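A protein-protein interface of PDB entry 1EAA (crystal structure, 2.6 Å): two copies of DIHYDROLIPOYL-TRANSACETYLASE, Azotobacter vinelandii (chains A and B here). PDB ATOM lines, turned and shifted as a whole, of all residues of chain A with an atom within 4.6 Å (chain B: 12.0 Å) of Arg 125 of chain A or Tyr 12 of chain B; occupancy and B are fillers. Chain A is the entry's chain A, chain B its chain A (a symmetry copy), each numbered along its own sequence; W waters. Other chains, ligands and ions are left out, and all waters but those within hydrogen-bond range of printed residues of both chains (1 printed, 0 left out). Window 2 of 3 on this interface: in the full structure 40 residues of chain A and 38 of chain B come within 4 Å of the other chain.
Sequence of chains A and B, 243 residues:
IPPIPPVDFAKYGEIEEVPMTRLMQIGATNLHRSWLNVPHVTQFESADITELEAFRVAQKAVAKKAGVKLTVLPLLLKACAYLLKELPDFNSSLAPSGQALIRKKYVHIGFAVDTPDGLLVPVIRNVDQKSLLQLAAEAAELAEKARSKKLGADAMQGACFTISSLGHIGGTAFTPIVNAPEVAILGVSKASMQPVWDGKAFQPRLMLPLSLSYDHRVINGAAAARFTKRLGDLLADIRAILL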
ATOM      1  N   TYR A 106      33.002 -27.144 -10.008  1.00  0.00           N
ATOM      2  CA  TYR A 106      32.758 -26.152 -11.035  1.00  0.00           C
ATOM      3  C   TYR A 106      32.952 -24.742 -10.481  1.00  0.00           C
ATOM      4  O   TYR A 106      32.881 -24.606  -9.258  1.00  0.00           O
ATOM      5  CB  TYR A 106      31.335 -26.336 -11.516  1.00  0.00           C
ATOM      6  CG  TYR A 106      30.203 -26.346 -10.474  1.00  0.00           C
ATOM      7  CD1 TYR A 106      29.825 -27.479  -9.745  1.00  0.00           C
ATOM      8  CD2 TYR A 106      29.464 -25.199 -10.351  1.00  0.00           C
ATOM      9  CE1 TYR A 106      28.699 -27.471  -8.941  1.00  0.00           C
ATOM     10  CE2 TYR A 106      28.344 -25.193  -9.559  1.00  0.00           C
ATOM     11  CZ  TYR A 106      27.966 -26.320  -8.883  1.00  0.00           C
ATOM     12  OH  TYR A 106      26.773 -26.244  -8.227  1.00  0.00           O
ATOM     13  N   VAL A 107      33.154 -23.649 -11.240  1.00  0.00           N
ATOM     14  CA  VAL A 107      33.365 -22.330 -10.645  1.00  0.00           C
ATOM     15  C   VAL A 107      32.449 -21.387 -11.409  1.00  0.00           C
ATOM     16  O   VAL A 107      32.691 -21.046 -12.568  1.00  0.00           O
ATOM     17  CB  VAL A 107      34.878 -21.842 -10.752  1.00  0.00           C
ATOM     18  CG1 VAL A 107      35.027 -20.531  -9.977  1.00  0.00           C
ATOM     19  CG2 VAL A 107      35.872 -22.848 -10.143  1.00  0.00           C
ATOM     20  N   HIS A 108      31.305 -21.031 -10.854  1.00  0.00           N
ATOM     21  CA  HIS A 108      30.471 -20.036 -11.495  1.00  0.00           C
ATOM     22  C   HIS A 108      30.421 -18.920 -10.419  1.00  0.00           C
ATOM     23  O   HIS A 108      30.331 -19.206  -9.210  1.00  0.00           O
ATOM     24  CB  HIS A 108      29.070 -20.553 -11.764  1.00  0.00           C
ATOM     25  CG  HIS A 108      28.876 -21.938 -12.381  1.00  0.00           C
ATOM     26  ND1 HIS A 108      27.783 -22.666 -12.228  1.00  0.00           N
ATOM     27  CD2 HIS A 108      29.733 -22.677 -13.163  1.00  0.00           C
ATOM     28  CE1 HIS A 108      27.931 -23.795 -12.867  1.00  0.00           C
ATOM     29  NE2 HIS A 108      29.103 -23.793 -13.428  1.00  0.00           N
ATOM     30  N   VAL A 123      25.059 -14.560 -12.932  1.00  0.00           N
ATOM     31  CA  VAL A 123      26.142 -15.513 -12.713  1.00  0.00           C
ATOM     32  C   VAL A 123      26.863 -15.759 -14.004  1.00  0.00           C
ATOM     33  O   VAL A 123      26.177 -15.910 -15.004  1.00  0.00           O
ATOM     34  CB  VAL A 123      25.544 -16.828 -12.192  1.00  0.00           C
ATOM     35  CG1 VAL A 123      26.541 -17.922 -11.952  1.00  0.00           C
ATOM     36  CG2 VAL A 123      24.894 -16.491 -10.886  1.00  0.00           C
ATOM     37  N   ILE A 124      28.186 -15.798 -14.022  1.00  0.00           N
ATOM     38  CA  ILE A 124      28.969 -16.172 -15.176  1.00  0.00           C
ATOM     39  C   ILE A 124      29.426 -17.601 -14.840  1.00  0.00           C
ATOM     40  O   ILE A 124      30.010 -17.868 -13.777  1.00  0.00           O
ATOM     41  CB  ILE A 124      30.161 -15.223 -15.311  1.00  0.00           C
ATOM     42  CG1 ILE A 124      29.643 -13.834 -15.507  1.00  0.00           C
ATOM     43  CG2 ILE A 124      31.050 -15.588 -16.486  1.00  0.00           C
ATOM     44  CD1 ILE A 124      30.771 -12.834 -15.657  1.00  0.00           C
ATOM     45  N   ARG A 125      29.149 -18.562 -15.725  1.00  0.00           N
ATOM     46  CA  ARG A 125      29.413 -19.977 -15.547  1.00  0.00           C
ATOM     47  C   ARG A 125      30.802 -20.347 -15.993  1.00  0.00           C
ATOM     48  O   ARG A 125      31.288 -19.817 -16.963  1.00  0.00           O
ATOM     49  CB  ARG A 125      28.402 -20.797 -16.341  1.00  0.00           C
ATOM     50  CG  ARG A 125      26.890 -20.543 -16.080  1.00  0.00           C
ATOM     51  CD  ARG A 125      26.364 -21.103 -14.742  1.00  0.00           C
ATOM     52  NE  ARG A 125      25.025 -20.661 -14.303  1.00  0.00           N
ATOM     53  CZ  ARG A 125      23.913 -21.420 -14.406  1.00  0.00           C
ATOM     54  NH1 ARG A 125      23.936 -22.661 -14.932  1.00  0.00           N
ATOM     55  NH2 ARG A 125      22.745 -20.931 -13.973  1.00  0.00           N
ATOM     56  N   ASN A 126      31.493 -21.191 -15.244  1.00  0.00           N
ATOM     57  CA  ASN A 126      32.814 -21.709 -15.521  1.00  0.00           C
ATOM     58  C   ASN A 126      33.765 -20.573 -15.839  1.00  0.00           C
ATOM     59  O   ASN A 126      34.472 -20.532 -16.837  1.00  0.00           O
ATOM     60  CB  ASN A 126      32.831 -22.711 -16.679  1.00  0.00           C
ATOM     61  CG  ASN A 126      31.854 -23.871 -16.596  1.00  0.00           C
ATOM     62  OD1 ASN A 126      31.996 -24.804 -15.798  1.00  0.00           O
ATOM     63  ND2 ASN A 126      30.794 -23.846 -17.403  1.00  0.00           N
ATOM     64  N   VAL A 127      33.904 -19.667 -14.868  1.00  0.00           N
ATOM     65  CA  VAL A 127      34.762 -18.502 -14.993  1.00  0.00           C
ATOM     66  C   VAL A 127      36.170 -19.000 -15.174  1.00  0.00           C
ATOM     67  O   VAL A 127      36.923 -18.429 -15.943  1.00  0.00           O
ATOM     68  CB  VAL A 127      34.672 -17.632 -13.751  1.00  0.00           C
ATOM     69  CG1 VAL A 127      35.721 -16.536 -13.766  1.00  0.00           C
ATOM     70  CG2 VAL A 127      33.313 -16.968 -13.738  1.00  0.00           C
ATOM     71  N   LYS A 130      37.257 -19.099 -18.916  1.00  0.00           N
ATOM     72  CA  LYS A 130      37.143 -18.026 -19.878  1.00  0.00           C
ATOM     73  C   LYS A 130      38.286 -17.035 -19.775  1.00  0.00           C
ATOM     74  O   LYS A 130      38.925 -16.888 -18.754  1.00  0.00           O
ATOM     75  CB  LYS A 130      35.819 -17.353 -19.674  1.00  0.00           C
ATOM     76  CG  LYS A 130      34.715 -18.363 -19.951  1.00  0.00           C
ATOM     77  CD  LYS A 130      33.336 -17.779 -19.678  1.00  0.00           C
ATOM     78  CE  LYS A 130      32.225 -18.805 -19.900  1.00  0.00           C
ATOM     79  NZ  LYS A 130      30.899 -18.279 -19.575  1.00  0.00           N
ATOM     80  N   ASP A 154      17.200 -18.202 -15.068  1.00  0.00           N
ATOM     81  CA  ASP A 154      18.232 -19.207 -15.261  1.00  0.00           C
ATOM     82  C   ASP A 154      19.571 -18.576 -14.903  1.00  0.00           C
ATOM     83  O   ASP A 154      20.325 -19.153 -14.132  1.00  0.00           O
ATOM     84  CB  ASP A 154      18.208 -19.656 -16.738  1.00  0.00           C
ATOM     85  CG  ASP A 154      19.325 -20.584 -17.267  1.00  0.00           C
ATOM     86  OD1 ASP A 154      19.552 -21.672 -16.718  1.00  0.00           O
ATOM     87  OD2 ASP A 154      19.972 -20.227 -18.260  1.00  0.00           O
ATOM     88  N   GLN A 157      21.229 -18.282 -11.256  1.00  0.00           N
ATOM     89  CA  GLN A 157      21.325 -19.482 -10.506  1.00  0.00           C
ATOM     90  C   GLN A 157      22.635 -20.211 -10.490  1.00  0.00           C
ATOM     91  O   GLN A 157      23.488 -20.085 -11.359  1.00  0.00           O
ATOM     92  CB  GLN A 157      20.189 -20.340 -10.990  1.00  0.00           C
ATOM     93  CG  GLN A 157      19.087 -20.051  -9.955  1.00  0.00           C
ATOM     94  CD  GLN A 157      17.698 -19.662 -10.469  1.00  0.00           C
ATOM     95  OE1 GLN A 157      17.200 -18.527 -10.328  1.00  0.00           O
ATOM     96  NE2 GLN A 157      16.998 -20.644 -11.037  1.00  0.00           N
ATOM     97  N   GLY A 158      22.781 -20.844  -9.327  1.00  0.00           N
ATOM     98  CA  GLY A 158      23.871 -21.757  -9.000  1.00  0.00           C
ATOM     99  C   GLY A 158      25.277 -21.231  -9.100  1.00  0.00           C
ATOM    100  O   GLY A 158      26.108 -21.800  -9.801  1.00  0.00           O
ATOM    101  N   PRO B   5      16.350 -22.389   1.861  1.00  0.00           N
ATOM    102  CA  PRO B   5      15.967 -23.310   0.812  1.00  0.00           C
ATOM    103  C   PRO B   5      17.131 -24.189   0.362  1.00  0.00           C
ATOM    104  O   PRO B   5      18.258 -23.712   0.143  1.00  0.00           O
ATOM    105  CB  PRO B   5      15.447 -22.412  -0.250  1.00  0.00           C
ATOM    106  CG  PRO B   5      14.744 -21.365   0.572  1.00  0.00           C
ATOM    107  CD  PRO B   5      15.815 -21.064   1.580  1.00  0.00           C
ATOM    108  N   PRO B   6      16.928 -25.508   0.304  1.00  0.00           N
ATOM    109  CA  PRO B   6      17.890 -26.458  -0.266  1.00  0.00           C
ATOM    110  C   PRO B   6      18.000 -26.284  -1.782  1.00  0.00           C
ATOM    111  O   PRO B   6      16.983 -26.099  -2.458  1.00  0.00           O
ATOM    112  CB  PRO B   6      17.359 -27.811   0.166  1.00  0.00           C
ATOM    113  CG  PRO B   6      15.870 -27.546   0.181  1.00  0.00           C
ATOM    114  CD  PRO B   6      15.799 -26.205   0.900  1.00  0.00           C
ATOM    115  N   VAL B   7      19.206 -26.309  -2.346  1.00  0.00           N
ATOM    116  CA  VAL B   7      19.400 -26.115  -3.774  1.00  0.00           C
ATOM    117  C   VAL B   7      19.908 -27.456  -4.303  1.00  0.00           C
ATOM    118  O   VAL B   7      20.618 -28.104  -3.525  1.00  0.00           O
ATOM    119  CB  VAL B   7      20.421 -25.003  -3.936  1.00  0.00           C
ATOM    120  CG1 VAL B   7      20.680 -24.751  -5.408  1.00  0.00           C
ATOM    121  CG2 VAL B   7      19.922 -23.756  -3.218  1.00  0.00           C
ATOM    122  N   ASP B   8      19.626 -27.984  -5.515  1.00  0.00           N
ATOM    123  CA  ASP B   8      20.231 -29.266  -5.933  1.00  0.00           C
ATOM    124  C   ASP B   8      21.535 -28.839  -6.584  1.00  0.00           C
ATOM    125  O   ASP B   8      21.537 -28.357  -7.717  1.00  0.00           O
ATOM    126  CB  ASP B   8      19.329 -30.049  -6.963  1.00  0.00           C
ATOM    127  CG  ASP B   8      19.672 -31.527  -7.405  1.00  0.00           C
ATOM    128  OD1 ASP B   8      20.837 -31.984  -7.318  1.00  0.00           O
ATOM    129  OD2 ASP B   8      18.717 -32.227  -7.856  1.00  0.00           O
ATOM    130  N   PHE B   9      22.669 -28.995  -5.910  1.00  0.00           N
ATOM    131  CA  PHE B   9      23.869 -28.359  -6.445  1.00  0.00           C
ATOM    132  C   PHE B   9      24.467 -29.058  -7.607  1.00  0.00           C
ATOM    133  O   PHE B   9      25.208 -28.435  -8.348  1.00  0.00           O
ATOM    134  CB  PHE B   9      25.012 -28.214  -5.432  1.00  0.00           C
ATOM    135  CG  PHE B   9      24.671 -27.197  -4.347  1.00  0.00           C
ATOM    136  CD1 PHE B   9      24.409 -25.884  -4.672  1.00  0.00           C
ATOM    137  CD2 PHE B   9      24.562 -27.608  -3.039  1.00  0.00           C
ATOM    138  CE1 PHE B   9      24.038 -25.014  -3.681  1.00  0.00           C
ATOM    139  CE2 PHE B   9      24.188 -26.733  -2.052  1.00  0.00           C
ATOM    140  CZ  PHE B   9      23.926 -25.433  -2.373  1.00  0.00           C
ATOM    141  N   ALA B  10      24.104 -30.316  -7.852  1.00  0.00           N
ATOM    142  CA  ALA B  10      24.699 -31.032  -8.953  1.00  0.00           C
ATOM    143  C   ALA B  10      24.000 -30.662 -10.237  1.00  0.00           C
ATOM    144  O   ALA B  10      24.404 -31.142 -11.274  1.00  0.00           O
ATOM    145  CB  ALA B  10      24.568 -32.494  -8.724  1.00  0.00           C
ATOM    146  N   LYS B  11      22.970 -29.815 -10.270  1.00  0.00           N
ATOM    147  CA  LYS B  11      22.383 -29.411 -11.535  1.00  0.00           C
ATOM    148  C   LYS B  11      23.350 -28.533 -12.307  1.00  0.00           C
ATOM    149  O   LYS B  11      23.192 -28.383 -13.524  1.00  0.00           O
ATOM    150  CB  LYS B  11      21.138 -28.566 -11.402  1.00  0.00           C
ATOM    151  CG  LYS B  11      19.975 -29.156 -10.636  1.00  0.00           C
ATOM    152  CD  LYS B  11      18.740 -28.237 -10.717  1.00  0.00           C
ATOM    153  CE  LYS B  11      17.604 -28.766  -9.806  1.00  0.00           C
ATOM    154  NZ  LYS B  11      16.357 -29.131 -10.485  1.00  0.00           N
ATOM    155  N   TYR B  12      24.321 -27.882 -11.622  1.00  0.00           N
ATOM    156  CA  TYR B  12      25.197 -26.894 -12.228  1.00  0.00           C
ATOM    157  C   TYR B  12      26.555 -27.475 -12.498  1.00  0.00           C
ATOM    158  O   TYR B  12      27.314 -26.785 -13.182  1.00  0.00           O
ATOM    159  CB  TYR B  12      25.337 -25.690 -11.319  1.00  0.00           C
ATOM    160  CG  TYR B  12      23.977 -25.144 -10.946  1.00  0.00           C
ATOM    161  CD1 TYR B  12      23.262 -24.527 -11.923  1.00  0.00           C
ATOM    162  CD2 TYR B  12      23.413 -25.329  -9.696  1.00  0.00           C
ATOM    163  CE1 TYR B  12      21.990 -24.070 -11.681  1.00  0.00           C
ATOM    164  CE2 TYR B  12      22.131 -24.874  -9.433  1.00  0.00           C
ATOM    165  CZ  TYR B  12      21.442 -24.245 -10.441  1.00  0.00           C
ATOM    166  OH  TYR B  12      20.157 -23.792 -10.260  1.00  0.00           O
ATOM    167  N   GLY B  13      26.927 -28.663 -12.016  1.00  0.00           N
ATOM    168  CA  GLY B  13      28.220 -29.261 -12.293  1.00  0.00           C
ATOM    169  C   GLY B  13      28.488 -30.424 -11.334  1.00  0.00           C
ATOM    170  O   GLY B  13      27.633 -30.814 -10.544  1.00  0.00           O
ATOM    171  N   GLU B  14      29.697 -30.970 -11.337  1.00  0.00           N
ATOM    172  CA  GLU B  14      30.092 -32.090 -10.502  1.00  0.00           C
ATOM    173  C   GLU B  14      30.201 -31.699  -9.028  1.00  0.00           C
ATOM    174  O   GLU B  14      30.789 -30.671  -8.738  1.00  0.00           O
ATOM    175  CB  GLU B  14      31.417 -32.565 -11.073  1.00  0.00           C
ATOM    176  CG  GLU B  14      31.609 -34.057 -11.438  1.00  0.00           C
ATOM    177  CD  GLU B  14      32.060 -35.053 -10.284  1.00  0.00           C
ATOM    178  OE1 GLU B  14      31.183 -35.598  -9.552  1.00  0.00           O
ATOM    179  OE2 GLU B  14      33.291 -35.313 -10.119  1.00  0.00           O
ATOM    180  N   ILE B  15      29.681 -32.395  -8.041  1.00  0.00           N
ATOM    181  CA  ILE B  15      29.861 -32.014  -6.666  1.00  0.00           C
ATOM    182  C   ILE B  15      30.449 -33.228  -6.004  1.00  0.00           C
ATOM    183  O   ILE B  15      30.461 -34.339  -6.537  1.00  0.00           O
ATOM    184  CB  ILE B  15      28.569 -31.687  -5.924  1.00  0.00           C
ATOM    185  CG1 ILE B  15      27.598 -32.845  -5.958  1.00  0.00           C
ATOM    186  CG2 ILE B  15      27.990 -30.436  -6.527  1.00  0.00           C
ATOM    187  CD1 ILE B  15      26.411 -32.670  -4.994  1.00  0.00           C
ATOM    188  N   GLU B  16      30.847 -33.005  -4.780  1.00  0.00           N
ATOM    189  CA  GLU B  16      31.488 -34.023  -4.011  1.00  0.00           C
ATOM    190  C   GLU B  16      31.197 -33.731  -2.562  1.00  0.00           C
ATOM    191  O   GLU B  16      31.404 -32.598  -2.168  1.00  0.00           O
ATOM    192  CB  GLU B  16      32.932 -33.923  -4.305  1.00  0.00           C
ATOM    193  CG  GLU B  16      33.781 -34.768  -3.386  1.00  0.00           C
ATOM    194  CD  GLU B  16      35.239 -34.419  -3.484  1.00  0.00           C
ATOM    195  OE1 GLU B  16      35.583 -33.246  -3.666  1.00  0.00           O
ATOM    196  OE2 GLU B  16      36.044 -35.348  -3.370  1.00  0.00           O
HETATM  197  O   HOH W   1      28.132 -25.514 -16.258  1.00  0.00           O
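ND1 of His 108 of chain A is in hydrogen-bond range of O of Gly 158 of chain A (3.1 Å).
The backbone carbonyl oxygen (O) of Arg 125 of chain A sits at hydrogen-bond distance from the side-chain amino group (NZ) of Lys 130 of chain A, at 3.1 Å.
O of Asp 154 of chain A lies within hydrogen-bond range of NH2 of Arg 125 of chain A, at 3.0 Å.
The guanidinium group (NH2) of Arg 125 of chain A is in hydrogen-bond range of the backbone carbonyl oxygen (O) of Gln 157 of chain A (2.8 Å).
OH of Tyr 106 of chain A is in hydrogen-bond range of O of Phe 9 of chain B (2.7 Å).
NE2 of His 108 of chain A lies close to O of Tyr 12 of chain B, at 3.5 Å.
Water W1 lies within hydrogen-bond range of ND2 of Asn 126 of chain A (3.3 Å), O of Tyr 12 of chain B (3.4 Å) and NE2 of His 108 of chain A (3.5 Å).
Among the printed residues, pairs that only touch across the chains: Tyr 106 of chain A with Tyr 12 of chain B (3.5 Å), Tyr 106 of chain A with Gly 13 of chain B (3.5 Å), Tyr 106 of chain A with Glu 14 of chain B (3.5 Å), Tyr 106 of chain A with Ile 15 of chain B (3.9 Å), Arg 125 of chain A with Tyr 12 of chain B (3.6 Å), Gln 157 of chain A with Tyr 12 of chain B (3.5 Å) and Gly 158 of chain A with Tyr 12 of chain B (3.6 Å).
No position is printed for both chains.
Of the 9 pairs that touch across the chains among the printed residues, none has its exchanged pair printed and touching as well.
Of the 12 printed residues of chain A, 5 touch a printed residue of chain B.
Hydrophobic or aromatic side chains of chain A that line the printed part of chain B: Tyr 106 and His 108.
Along chain A the printed residues that touch a printed residue of chain B span positions 106 to 158.
Hydrophobic or aromatic side chains of chain B that line the printed part of chain A: Phe 9, Tyr 12 and Ile 15.
Among the printed residues, 9 pairs touch across the chains.
Of chain B, only Tyr 12 comes within 4 Å of Arg 125 of chain A.
Tyr 12 of chain B touches just these residues of chain A: Tyr 106 (3.5 Å), His 108 (3.1 Å), Arg 125 (3.6 Å), Gln 157 (3.5 Å) and Gly 158 (3.6 Å).
Tyr 106 of chain A touches just these residues of chain B: Phe 9 (2.7 Å), Tyr 12 (3.5 Å), Gly 13 (3.5 Å), Glu 14 (3.5 Å) and Ile 15 (3.9 Å).
His 108 of chain A touches one residue of chain B.
Val 123 of chain A touches none of the printed residues of chain B.
No residue of chain B comes within 4 Å of Ile 124 of chain A.
No residue of chain B comes within 4 Å of Val 127 of chain A.
No residue of chain B comes within 4 Å of Asp 154 of chain A.
Of chain B, only Tyr 12 comes within 4 Å of Gln 157 of chain A.
Of the printed residues of chain A, Gly 13 of chain B touches Tyr 106 (3.5 Å).
Of the printed residues of chain A, Glu 14 of chain B touches Tyr 106.
Of the printed residues of chain A, Phe 9 of chain B touches Tyr 106 (2.7 Å).
Pro 5 of chain B touches none of the printed residues of chain A.
The nearest printed residue of chain A that does not touch Gly 13 of chain B is His 108 of chain A (5.0 Å).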
